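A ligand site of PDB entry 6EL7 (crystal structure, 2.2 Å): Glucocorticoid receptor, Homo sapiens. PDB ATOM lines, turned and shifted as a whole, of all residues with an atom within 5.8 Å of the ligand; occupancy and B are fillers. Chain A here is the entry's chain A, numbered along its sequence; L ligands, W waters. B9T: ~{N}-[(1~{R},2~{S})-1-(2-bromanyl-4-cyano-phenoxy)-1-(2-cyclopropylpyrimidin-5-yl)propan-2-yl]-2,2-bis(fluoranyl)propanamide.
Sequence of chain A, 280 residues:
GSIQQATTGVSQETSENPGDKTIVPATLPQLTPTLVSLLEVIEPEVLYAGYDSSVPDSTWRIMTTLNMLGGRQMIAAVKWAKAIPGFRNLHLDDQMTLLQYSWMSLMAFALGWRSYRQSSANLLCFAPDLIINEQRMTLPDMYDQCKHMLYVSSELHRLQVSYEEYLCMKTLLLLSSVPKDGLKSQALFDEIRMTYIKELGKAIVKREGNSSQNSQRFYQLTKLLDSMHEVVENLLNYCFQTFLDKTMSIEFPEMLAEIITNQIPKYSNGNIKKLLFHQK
The guanidinium group (NH2) of Arg 114 sits at hydrogen-bond distance from a nitrogen (N24) of the ligand, 3.0 Å away. The side-chain amide nitrogen (NE2) of Gln 145 is in hydrogen-bond range of an oxygen (O27) of the ligand (2.9 Å). NE2 of Gln 73 is in hydrogen-bond range of N24 of the ligand, 2.9 Å away. A nitrogen (N25) of the ligand is in hydrogen-bond range of the side-chain amide oxygen of Asn 67 (2.8 Å).
The backbone carbonyl oxygen of Phe 126 sits at hydrogen-bond distance from the guanidinium group of Arg 114, 2.9 Å away. The side-chain hydroxyl (OG1) of Thr 242 sits at hydrogen-bond distance from the backbone carbonyl oxygen (O) of Tyr 238 (2.9 Å). NE2 of Gln 145 lies within hydrogen-bond range of O of Leu 235 (3.0 Å). SG of Cys 146 sits at hydrogen-bond distance from O of Met 142 (3.4 Å).
Residues that only touch the ligand: Met 63, Leu 66, Leu 69, Gly 70, Trp 103, Met 104, Met 107, Phe 126, Met 142, Cys 146, Met 149, Tyr 238, Cys 239, Thr 242, Ile 250 and Phe 252. Hydrophobic or aromatic side chains that line the ligand: Met 63, Leu 66, Leu 69, Trp 103, Met 104, Met 107, Phe 126, Met 142, Met 149, Tyr 238, Ile 250 and Phe 252. Of the 32 residues printed, 20 come within 4 Å of the ligand.
Water W1 lies within hydrogen-bond range of O of Met 107 (2.8 Å), NH2 of Arg 114 (3.0 Å) and N24 of the ligand (3.4 Å).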
ATOM      1  N   ILE A  62      11.802  -0.271 -20.629  1.00  0.00           N
ATOM      2  CA  ILE A  62      12.538  -1.536 -20.479  1.00  0.00           C
ATOM      3  C   ILE A  62      13.994  -1.265 -20.091  1.00  0.00           C
ATOM      4  O   ILE A  62      14.483  -1.864 -19.130  1.00  0.00           O
ATOM      5  CB  ILE A  62      12.382  -2.446 -21.735  1.00  0.00           C
ATOM      6  CG1 ILE A  62      10.937  -3.034 -21.786  1.00  0.00           C
ATOM      7  CG2 ILE A  62      13.437  -3.562 -21.766  1.00  0.00           C
ATOM      8  CD1 ILE A  62      10.481  -3.666 -23.122  1.00  0.00           C
ATOM      9  N   MET A  63      14.660  -0.316 -20.775  1.00  0.00           N
ATOM     10  CA  MET A  63      16.045   0.061 -20.484  1.00  0.00           C
ATOM     11  C   MET A  63      16.192   0.571 -19.061  1.00  0.00           C
ATOM     12  O   MET A  63      17.170   0.200 -18.428  1.00  0.00           O
ATOM     13  CB  MET A  63      16.564   1.115 -21.457  1.00  0.00           C
ATOM     14  CG  MET A  63      16.856   0.547 -22.824  1.00  0.00           C
ATOM     15  SD  MET A  63      17.394   1.866 -23.937  1.00  0.00           S
ATOM     16  CE  MET A  63      17.895   0.854 -25.404  1.00  0.00           C
ATOM     17  N   THR A  64      15.209   1.389 -18.570  1.00  0.00           N
ATOM     18  CA  THR A  64      15.209   1.917 -17.183  1.00  0.00           C
ATOM     19  C   THR A  64      15.103   0.767 -16.164  1.00  0.00           C
ATOM     20  O   THR A  64      15.935   0.699 -15.281  1.00  0.00           O
ATOM     21  CB  THR A  64      14.089   2.962 -16.979  1.00  0.00           C
ATOM     22  OG1 THR A  64      14.272   4.010 -17.942  1.00  0.00           O
ATOM     23  CG2 THR A  64      14.078   3.558 -15.557  1.00  0.00           C
ATOM     24  N   LEU A  66      15.715  -2.455 -16.630  1.00  0.00           N
ATOM     25  CA  LEU A  66      16.901  -3.299 -16.732  1.00  0.00           C
ATOM     26  C   LEU A  66      18.128  -2.660 -16.067  1.00  0.00           C
ATOM     27  O   LEU A  66      18.962  -3.380 -15.497  1.00  0.00           O
ATOM     28  CB  LEU A  66      17.187  -3.720 -18.173  1.00  0.00           C
ATOM     29  CG  LEU A  66      16.172  -4.708 -18.812  1.00  0.00           C
ATOM     30  CD1 LEU A  66      16.561  -5.024 -20.239  1.00  0.00           C
ATOM     31  CD2 LEU A  66      16.087  -6.002 -18.011  1.00  0.00           C
ATOM     32  N   ASN A  67      18.225  -1.325 -16.066  1.00  0.00           N
ATOM     33  CA  ASN A  67      19.333  -0.654 -15.362  1.00  0.00           C
ATOM     34  C   ASN A  67      19.158  -0.885 -13.864  1.00  0.00           C
ATOM     35  O   ASN A  67      20.128  -1.209 -13.175  1.00  0.00           O
ATOM     36  CB  ASN A  67      19.378   0.849 -15.699  1.00  0.00           C
ATOM     37  CG  ASN A  67      20.027   1.158 -17.018  1.00  0.00           C
ATOM     38  OD1 ASN A  67      20.684   0.332 -17.627  1.00  0.00           O
ATOM     39  ND2 ASN A  67      19.829   2.375 -17.500  1.00  0.00           N
ATOM     40  N   LEU A  69      17.534  -3.423 -12.384  1.00  0.00           N
ATOM     41  CA  LEU A  69      17.823  -4.839 -12.209  1.00  0.00           C
ATOM     42  C   LEU A  69      19.369  -5.083 -12.218  1.00  0.00           C
ATOM     43  O   LEU A  69      19.867  -5.823 -11.377  1.00  0.00           O
ATOM     44  CB  LEU A  69      17.125  -5.670 -13.312  1.00  0.00           C
ATOM     45  CG  LEU A  69      17.451  -7.199 -13.336  1.00  0.00           C
ATOM     46  CD1 LEU A  69      16.871  -7.900 -12.082  1.00  0.00           C
ATOM     47  CD2 LEU A  69      16.940  -7.846 -14.636  1.00  0.00           C
ATOM     48  N   GLY A  70      20.059  -4.426 -13.153  1.00  0.00           N
ATOM     49  CA  GLY A  70      21.516  -4.478 -13.295  1.00  0.00           C
ATOM     50  C   GLY A  70      22.258  -4.039 -12.039  1.00  0.00           C
ATOM     51  O   GLY A  70      23.250  -4.633 -11.668  1.00  0.00           O
ATOM     52  N   GLN A  73      21.859  -6.808  -9.489  1.00  0.00           N
ATOM     53  CA  GLN A  73      22.717  -7.930  -9.900  1.00  0.00           C
ATOM     54  C   GLN A  73      24.159  -7.633  -9.510  1.00  0.00           C
ATOM     55  O   GLN A  73      24.853  -8.536  -9.041  1.00  0.00           O
ATOM     56  CB  GLN A  73      22.645  -8.160 -11.423  1.00  0.00           C
ATOM     57  CG  GLN A  73      21.249  -8.526 -11.947  1.00  0.00           C
ATOM     58  CD  GLN A  73      20.934 -10.009 -12.043  1.00  0.00           C
ATOM     59  OE1 GLN A  73      21.526 -10.876 -11.395  1.00  0.00           O
ATOM     60  NE2 GLN A  73      19.937 -10.328 -12.862  1.00  0.00           N
ATOM     61  N   TRP A 103      32.214  -6.014 -14.557  1.00  0.00           N
ATOM     62  CA  TRP A 103      30.774  -5.850 -14.317  1.00  0.00           C
ATOM     63  C   TRP A 103      29.907  -6.285 -15.504  1.00  0.00           C
ATOM     64  O   TRP A 103      29.088  -7.186 -15.360  1.00  0.00           O
ATOM     65  CB  TRP A 103      30.407  -4.413 -13.854  1.00  0.00           C
ATOM     66  CG  TRP A 103      30.543  -3.329 -14.893  1.00  0.00           C
ATOM     67  CD1 TRP A 103      31.679  -2.893 -15.485  1.00  0.00           C
ATOM     68  CD2 TRP A 103      29.472  -2.539 -15.455  1.00  0.00           C
ATOM     69  NE1 TRP A 103      31.393  -1.925 -16.413  1.00  0.00           N
ATOM     70  CE2 TRP A 103      30.054  -1.655 -16.389  1.00  0.00           C
ATOM     71  CE3 TRP A 103      28.081  -2.512 -15.274  1.00  0.00           C
ATOM     72  CZ2 TRP A 103      29.295  -0.728 -17.114  1.00  0.00           C
ATOM     73  CZ3 TRP A 103      27.329  -1.623 -16.014  1.00  0.00           C
ATOM     74  CH2 TRP A 103      27.931  -0.730 -16.909  1.00  0.00           C
ATOM     75  N   MET A 104      30.109  -5.680 -16.663  1.00  0.00           N
ATOM     76  CA  MET A 104      29.333  -5.949 -17.871  1.00  0.00           C
ATOM     77  C   MET A 104      29.593  -7.365 -18.433  1.00  0.00           C
ATOM     78  O   MET A 104      28.647  -7.984 -18.913  1.00  0.00           O
ATOM     79  CB  MET A 104      29.583  -4.838 -18.924  1.00  0.00           C
ATOM     80  CG  MET A 104      28.747  -5.011 -20.196  1.00  0.00           C
ATOM     81  SD  MET A 104      26.965  -4.857 -19.858  1.00  0.00           S
ATOM     82  CE  MET A 104      26.805  -3.058 -19.974  1.00  0.00           C
ATOM     83  N   MET A 107      27.489  -9.680 -16.177  1.00  0.00           N
ATOM     84  CA  MET A 107      26.058  -9.561 -16.439  1.00  0.00           C
ATOM     85  C   MET A 107      25.648 -10.170 -17.785  1.00  0.00           C
ATOM     86  O   MET A 107      24.668 -10.911 -17.817  1.00  0.00           O
ATOM     87  CB  MET A 107      25.608  -8.109 -16.317  1.00  0.00           C
ATOM     88  CG  MET A 107      25.693  -7.605 -14.877  1.00  0.00           C
ATOM     89  SD  MET A 107      24.873  -6.018 -14.731  1.00  0.00           S
ATOM     90  CE  MET A 107      25.886  -5.029 -15.696  1.00  0.00           C
ATOM     91  N   ALA A 108      26.391  -9.870 -18.867  1.00  0.00           N
ATOM     92  CA  ALA A 108      26.107 -10.403 -20.204  1.00  0.00           C
ATOM     93  C   ALA A 108      26.291 -11.930 -20.222  1.00  0.00           C
ATOM     94  O   ALA A 108      25.485 -12.652 -20.827  1.00  0.00           O
ATOM     95  CB  ALA A 108      27.029  -9.741 -21.229  1.00  0.00           C
ATOM     96  N   LEU A 111      23.516 -13.531 -18.243  1.00  0.00           N
ATOM     97  CA  LEU A 111      22.291 -13.344 -19.040  1.00  0.00           C
ATOM     98  C   LEU A 111      22.257 -14.352 -20.196  1.00  0.00           C
ATOM     99  O   LEU A 111      21.204 -14.956 -20.444  1.00  0.00           O
ATOM    100  CB  LEU A 111      22.158 -11.888 -19.545  1.00  0.00           C
ATOM    101  CG  LEU A 111      21.161 -11.674 -20.728  1.00  0.00           C
ATOM    102  CD1 LEU A 111      19.711 -11.836 -20.266  1.00  0.00           C
ATOM    103  CD2 LEU A 111      21.343 -10.339 -21.388  1.00  0.00           C
ATOM    104  N   ARG A 114      21.256 -17.780 -18.762  1.00  0.00           N
ATOM    105  CA  ARG A 114      19.818 -17.872 -18.466  1.00  0.00           C
ATOM    106  C   ARG A 114      19.020 -18.011 -19.750  1.00  0.00           C
ATOM    107  O   ARG A 114      18.092 -18.803 -19.786  1.00  0.00           O
ATOM    108  CB  ARG A 114      19.300 -16.636 -17.692  1.00  0.00           C
ATOM    109  CG  ARG A 114      19.818 -16.540 -16.279  1.00  0.00           C
ATOM    110  CD  ARG A 114      19.073 -15.492 -15.446  1.00  0.00           C
ATOM    111  NE  ARG A 114      19.127 -14.123 -15.986  1.00  0.00           N
ATOM    112  CZ  ARG A 114      20.119 -13.261 -15.799  1.00  0.00           C
ATOM    113  NH1 ARG A 114      21.232 -13.645 -15.185  1.00  0.00           N
ATOM    114  NH2 ARG A 114      20.038 -12.039 -16.275  1.00  0.00           N
ATOM    115  N   LEU A 124      15.977 -13.029 -24.850  1.00  0.00           N
ATOM    116  CA  LEU A 124      16.907 -12.611 -23.814  1.00  0.00           C
ATOM    117  C   LEU A 124      16.155 -12.717 -22.491  1.00  0.00           C
ATOM    118  O   LEU A 124      15.160 -12.013 -22.285  1.00  0.00           O
ATOM    119  CB  LEU A 124      17.495 -11.216 -24.060  1.00  0.00           C
ATOM    120  CG  LEU A 124      18.592 -11.121 -25.138  1.00  0.00           C
ATOM    121  CD1 LEU A 124      19.030  -9.701 -25.333  1.00  0.00           C
ATOM    122  CD2 LEU A 124      19.828 -12.022 -24.819  1.00  0.00           C
ATOM    123  N   PHE A 126      16.355 -11.789 -19.199  1.00  0.00           N
ATOM    124  CA  PHE A 126      16.922 -10.894 -18.173  1.00  0.00           C
ATOM    125  C   PHE A 126      16.440 -11.270 -16.769  1.00  0.00           C
ATOM    126  O   PHE A 126      17.221 -11.302 -15.822  1.00  0.00           O
ATOM    127  CB  PHE A 126      16.569  -9.431 -18.469  1.00  0.00           C
ATOM    128  CG  PHE A 126      17.356  -8.807 -19.595  1.00  0.00           C
ATOM    129  CD1 PHE A 126      18.568  -8.179 -19.357  1.00  0.00           C
ATOM    130  CD2 PHE A 126      16.854  -8.820 -20.897  1.00  0.00           C
ATOM    131  CE1 PHE A 126      19.295  -7.583 -20.400  1.00  0.00           C
ATOM    132  CE2 PHE A 126      17.566  -8.198 -21.938  1.00  0.00           C
ATOM    133  CZ  PHE A 126      18.792  -7.624 -21.689  1.00  0.00           C
ATOM    134  N   ALA A 127      15.140 -11.567 -16.671  1.00  0.00           N
ATOM    135  CA  ALA A 127      14.462 -11.935 -15.430  1.00  0.00           C
ATOM    136  C   ALA A 127      13.239 -12.794 -15.829  1.00  0.00           C
ATOM    137  O   ALA A 127      12.722 -12.635 -16.943  1.00  0.00           O
ATOM    138  CB  ALA A 127      13.985 -10.680 -14.702  1.00  0.00           C
ATOM    139  N   ILE A 132      12.934 -10.541 -23.155  1.00  0.00           N
ATOM    140  CA  ILE A 132      12.906  -9.802 -24.403  1.00  0.00           C
ATOM    141  C   ILE A 132      12.617 -10.801 -25.528  1.00  0.00           C
ATOM    142  O   ILE A 132      13.513 -11.509 -26.001  1.00  0.00           O
ATOM    143  CB  ILE A 132      14.120  -8.860 -24.648  1.00  0.00           C
ATOM    144  CG1 ILE A 132      14.276  -7.796 -23.506  1.00  0.00           C
ATOM    145  CG2 ILE A 132      14.072  -8.189 -26.049  1.00  0.00           C
ATOM    146  CD1 ILE A 132      13.038  -7.071 -23.025  1.00  0.00           C
ATOM    147  N   MET A 142      15.712  -1.140 -29.707  1.00  0.00           N
ATOM    148  CA  MET A 142      15.906  -2.304 -28.839  1.00  0.00           C
ATOM    149  C   MET A 142      17.030  -3.256 -29.289  1.00  0.00           C
ATOM    150  O   MET A 142      17.909  -3.592 -28.494  1.00  0.00           O
ATOM    151  CB  MET A 142      14.590  -3.095 -28.635  1.00  0.00           C
ATOM    152  CG  MET A 142      14.679  -4.106 -27.467  1.00  0.00           C
ATOM    153  SD  MET A 142      14.888  -3.306 -25.852  1.00  0.00           S
ATOM    154  CE  MET A 142      13.216  -2.889 -25.501  1.00  0.00           C
ATOM    155  N   GLN A 145      21.454  -3.023 -28.885  1.00  0.00           N
ATOM    156  CA  GLN A 145      22.136  -3.542 -27.719  1.00  0.00           C
ATOM    157  C   GLN A 145      21.941  -5.056 -27.606  1.00  0.00           C
ATOM    158  O   GLN A 145      22.897  -5.786 -27.358  1.00  0.00           O
ATOM    159  CB  GLN A 145      21.632  -2.799 -26.474  1.00  0.00           C
ATOM    160  CG  GLN A 145      22.578  -2.759 -25.279  1.00  0.00           C
ATOM    161  CD  GLN A 145      23.865  -1.982 -25.464  1.00  0.00           C
ATOM    162  OE1 GLN A 145      24.487  -1.980 -26.537  1.00  0.00           O
ATOM    163  NE2 GLN A 145      24.389  -1.463 -24.362  1.00  0.00           N
ATOM    164  N   CYS A 146      20.695  -5.521 -27.865  1.00  0.00           N
ATOM    165  CA  CYS A 146      20.257  -6.919 -27.783  1.00  0.00           C
ATOM    166  C   CYS A 146      21.054  -7.900 -28.639  1.00  0.00           C
ATOM    167  O   CYS A 146      21.275  -9.020 -28.187  1.00  0.00           O
ATOM    168  CB  CYS A 146      18.768  -7.042 -28.056  1.00  0.00           C
ATOM    169  SG  CYS A 146      17.743  -6.460 -26.694  1.00  0.00           S
ATOM    170  N   MET A 149      24.169  -9.294 -26.846  1.00  0.00           N
ATOM    171  CA  MET A 149      23.800 -10.235 -25.809  1.00  0.00           C
ATOM    172  C   MET A 149      23.286 -11.539 -26.425  1.00  0.00           C
ATOM    173  O   MET A 149      23.643 -12.615 -25.925  1.00  0.00           O
ATOM    174  CB  MET A 149      22.784  -9.605 -24.854  1.00  0.00           C
ATOM    175  CG  MET A 149      23.419  -8.523 -23.989  1.00  0.00           C
ATOM    176  SD  MET A 149      22.288  -7.452 -23.076  1.00  0.00           S
ATOM    177  CE  MET A 149      21.405  -6.683 -24.383  1.00  0.00           C
ATOM    178  N   LEU A 235      28.800  -3.277 -25.926  1.00  0.00           N
ATOM    179  CA  LEU A 235      27.781  -2.954 -24.896  1.00  0.00           C
ATOM    180  C   LEU A 235      28.136  -1.680 -24.139  1.00  0.00           C
ATOM    181  O   LEU A 235      27.256  -0.845 -23.905  1.00  0.00           O
ATOM    182  CB  LEU A 235      27.562  -4.110 -23.900  1.00  0.00           C
ATOM    183  CG  LEU A 235      26.896  -5.403 -24.435  1.00  0.00           C
ATOM    184  CD1 LEU A 235      27.047  -6.541 -23.454  1.00  0.00           C
ATOM    185  CD2 LEU A 235      25.430  -5.180 -24.787  1.00  0.00           C
ATOM    186  N   TYR A 238      27.663   1.878 -26.186  1.00  0.00           N
ATOM    187  CA  TYR A 238      26.269   2.265 -26.126  1.00  0.00           C
ATOM    188  C   TYR A 238      25.891   2.747 -24.723  1.00  0.00           C
ATOM    189  O   TYR A 238      25.266   3.792 -24.574  1.00  0.00           O
ATOM    190  CB  TYR A 238      25.428   1.047 -26.517  1.00  0.00           C
ATOM    191  CG  TYR A 238      23.984   1.308 -26.843  1.00  0.00           C
ATOM    192  CD1 TYR A 238      23.029   1.446 -25.838  1.00  0.00           C
ATOM    193  CD2 TYR A 238      23.539   1.317 -28.158  1.00  0.00           C
ATOM    194  CE1 TYR A 238      21.685   1.651 -26.135  1.00  0.00           C
ATOM    195  CE2 TYR A 238      22.194   1.507 -28.472  1.00  0.00           C
ATOM    196  CZ  TYR A 238      21.265   1.675 -27.452  1.00  0.00           C
ATOM    197  OH  TYR A 238      19.944   1.837 -27.771  1.00  0.00           O
ATOM    198  N   CYS A 239      26.249   1.949 -23.684  1.00  0.00           N
ATOM    199  CA  CYS A 239      25.966   2.215 -22.269  1.00  0.00           C
ATOM    200  C   CYS A 239      26.612   3.536 -21.745  1.00  0.00           C
ATOM    201  O   CYS A 239      25.969   4.285 -21.011  1.00  0.00           O
ATOM    202  CB  CYS A 239      26.372   1.024 -21.417  1.00  0.00           C
ATOM    203  SG  CYS A 239      26.225   1.312 -19.640  1.00  0.00           S
ATOM    204  N   PHE A 240      27.884   3.782 -22.100  1.00  0.00           N
ATOM    205  CA  PHE A 240      28.589   5.006 -21.712  1.00  0.00           C
ATOM    206  C   PHE A 240      27.934   6.235 -22.362  1.00  0.00           C
ATOM    207  O   PHE A 240      27.750   7.257 -21.699  1.00  0.00           O
ATOM    208  CB  PHE A 240      30.106   4.916 -22.077  1.00  0.00           C
ATOM    209  CG  PHE A 240      30.953   3.973 -21.244  1.00  0.00           C
ATOM    210  CD1 PHE A 240      30.480   3.456 -20.037  1.00  0.00           C
ATOM    211  CD2 PHE A 240      32.245   3.636 -21.634  1.00  0.00           C
ATOM    212  CE1 PHE A 240      31.286   2.611 -19.254  1.00  0.00           C
ATOM    213  CE2 PHE A 240      33.029   2.775 -20.866  1.00  0.00           C
ATOM    214  CZ  PHE A 240      32.562   2.293 -19.666  1.00  0.00           C
ATOM    215  N   THR A 242      24.754   6.570 -23.374  1.00  0.00           N
ATOM    216  CA  THR A 242      23.445   6.663 -22.727  1.00  0.00           C
ATOM    217  C   THR A 242      23.599   7.267 -21.319  1.00  0.00           C
ATOM    218  O   THR A 242      22.801   8.102 -20.928  1.00  0.00           O
ATOM    219  CB  THR A 242      22.757   5.274 -22.754  1.00  0.00           C
ATOM    220  OG1 THR A 242      22.649   4.856 -24.121  1.00  0.00           O
ATOM    221  CG2 THR A 242      21.363   5.309 -22.162  1.00  0.00           C
ATOM    222  N   PHE A 243      24.649   6.862 -20.581  1.00  0.00           N
ATOM    223  CA  PHE A 243      24.879   7.394 -19.237  1.00  0.00           C
ATOM    224  C   PHE A 243      25.244   8.885 -19.309  1.00  0.00           C
ATOM    225  O   PHE A 243      24.705   9.665 -18.538  1.00  0.00           O
ATOM    226  CB  PHE A 243      25.946   6.575 -18.491  1.00  0.00           C
ATOM    227  CG  PHE A 243      26.348   7.200 -17.171  1.00  0.00           C
ATOM    228  CD1 PHE A 243      25.602   6.968 -16.010  1.00  0.00           C
ATOM    229  CD2 PHE A 243      27.442   8.058 -17.081  1.00  0.00           C
ATOM    230  CE1 PHE A 243      25.948   7.578 -14.807  1.00  0.00           C
ATOM    231  CE2 PHE A 243      27.828   8.621 -15.861  1.00  0.00           C
ATOM    232  CZ  PHE A 243      27.076   8.375 -14.730  1.00  0.00           C
ATOM    233  N   ILE A 250      17.740   8.596 -19.099  1.00  0.00           N
ATOM    234  CA  ILE A 250      17.894   7.172 -18.791  1.00  0.00           C
ATOM    235  C   ILE A 250      18.573   7.094 -17.420  1.00  0.00           C
ATOM    236  O   ILE A 250      19.730   7.517 -17.259  1.00  0.00           O
ATOM    237  CB  ILE A 250      18.621   6.334 -19.887  1.00  0.00           C
ATOM    238  CG1 ILE A 250      17.770   6.216 -21.200  1.00  0.00           C
ATOM    239  CG2 ILE A 250      19.016   4.947 -19.368  1.00  0.00           C
ATOM    240  CD1 ILE A 250      16.652   5.124 -21.205  1.00  0.00           C
ATOM    241  N   PHE A 252      20.213   5.332 -14.074  1.00  0.00           N
ATOM    242  CA  PHE A 252      21.099   4.276 -13.640  1.00  0.00           C
ATOM    243  C   PHE A 252      21.087   4.331 -12.125  1.00  0.00           C
ATOM    244  O   PHE A 252      21.206   5.426 -11.558  1.00  0.00           O
ATOM    245  CB  PHE A 252      22.536   4.515 -14.151  1.00  0.00           C
ATOM    246  CG  PHE A 252      22.701   4.266 -15.637  1.00  0.00           C
ATOM    247  CD1 PHE A 252      22.309   5.219 -16.568  1.00  0.00           C
ATOM    248  CD2 PHE A 252      23.259   3.077 -16.099  1.00  0.00           C
ATOM    249  CE1 PHE A 252      22.423   4.969 -17.941  1.00  0.00           C
ATOM    250  CE2 PHE A 252      23.418   2.852 -17.464  1.00  0.00           C
ATOM    251  CZ  PHE A 252      23.000   3.805 -18.377  1.00  0.00           C
ATOM    252  N   LEU A 256      25.487   1.131 -10.522  1.00  0.00           N
ATOM    253  CA  LEU A 256      25.929   1.217 -11.918  1.00  0.00           C
ATOM    254  C   LEU A 256      26.525   2.573 -12.225  1.00  0.00           C
ATOM    255  O   LEU A 256      27.525   2.606 -12.929  1.00  0.00           O
ATOM    256  CB  LEU A 256      24.795   0.883 -12.904  1.00  0.00           C
ATOM    257  CG  LEU A 256      24.256  -0.569 -12.840  1.00  0.00           C
ATOM    258  CD1 LEU A 256      23.375  -0.868 -14.114  1.00  0.00           C
ATOM    259  CD2 LEU A 256      25.406  -1.615 -12.678  1.00  0.00           C
ATOM    260  N   ILE A 260      30.286   3.092 -13.754  1.00  0.00           N
ATOM    261  CA  ILE A 260      30.465   3.820 -15.013  1.00  0.00           C
ATOM    262  C   ILE A 260      31.356   5.060 -14.849  1.00  0.00           C
ATOM    263  O   ILE A 260      32.222   5.312 -15.680  1.00  0.00           O
ATOM    264  CB  ILE A 260      29.073   4.125 -15.649  1.00  0.00           C
ATOM    265  CG1 ILE A 260      28.383   2.794 -16.040  1.00  0.00           C
ATOM    266  CG2 ILE A 260      29.209   5.047 -16.892  1.00  0.00           C
ATOM    267  CD1 ILE A 260      26.858   2.959 -16.312  1.00  0.00           C
HETATM  268  C1  B9T L   1      23.919  -1.395 -18.045  1.00  0.00           C
HETATM  269  C2  B9T L   1      23.003  -1.670 -19.209  1.00  0.00           C
HETATM  270  C7  B9T L   1      19.736  -2.146 -19.936  1.00  0.00           C
HETATM  271  C9  B9T L   1      19.073  -3.030 -21.955  1.00  0.00           C
HETATM  272  C11 B9T L   1      21.099  -3.637 -21.111  1.00  0.00           C
HETATM  273  C12 B9T L   1      18.043  -3.115 -23.034  1.00  0.00           C
HETATM  274  C13 B9T L   1      17.734  -4.408 -23.728  1.00  0.00           C
HETATM  275  C14 B9T L   1      18.428  -3.305 -24.468  1.00  0.00           C
HETATM  276  C16 B9T L   1      22.076  -5.002 -18.120  1.00  0.00           C
HETATM  277  C19 B9T L   1      21.041  -7.177 -16.777  1.00  0.00           C
HETATM  278  C20 B9T L   1      22.074  -7.372 -17.675  1.00  0.00           C
HETATM  279  C21 B9T L   1      22.585  -6.279 -18.339  1.00  0.00           C
HETATM  280  N25 B9T L   1      22.434  -0.428 -19.702  1.00  0.00           N
HETATM  281  C4  B9T L   1      21.959  -2.739 -18.889  1.00  0.00           C
HETATM  282  C6  B9T L   1      20.929  -2.837 -19.985  1.00  0.00           C
HETATM  283  N8  B9T L   1      18.803  -2.226 -20.902  1.00  0.00           N
HETATM  284  N10 B9T L   1      20.199  -3.748 -22.087  1.00  0.00           N
HETATM  285  O15 B9T L   1      22.678  -3.969 -18.821  1.00  0.00           O
HETATM  286  C17 B9T L   1      21.054  -4.824 -17.213  1.00  0.00           C
HETATM  287  C18 B9T L   1      20.534  -5.914 -16.545  1.00  0.00           C
HETATM  288 BR2  B9T L   1      23.997  -6.531 -19.588  1.00  0.00          BR
HETATM  289  C23 B9T L   1      20.473  -8.269 -16.090  1.00  0.00           C
HETATM  290  N24 B9T L   1      19.974  -9.139 -15.506  1.00  0.00           N
HETATM  291  C26 B9T L   1      22.512  -0.113 -21.041  1.00  0.00           C
HETATM  292  O27 B9T L   1      23.181  -0.738 -21.865  1.00  0.00           O
HETATM  293  C28 B9T L   1      21.724   1.100 -21.476  1.00  0.00           C
HETATM  294  C29 B9T L   1      20.618   0.663 -22.416  1.00  0.00           C
HETATM  295  F30 B9T L   1      21.143   1.840 -20.499  1.00  0.00           F
HETATM  296  F31 B9T L   1      22.559   1.931 -22.167  1.00  0.00           F
HETATM  297  O   HOH W   1      22.823 -10.916 -15.774  1.00  0.00           O
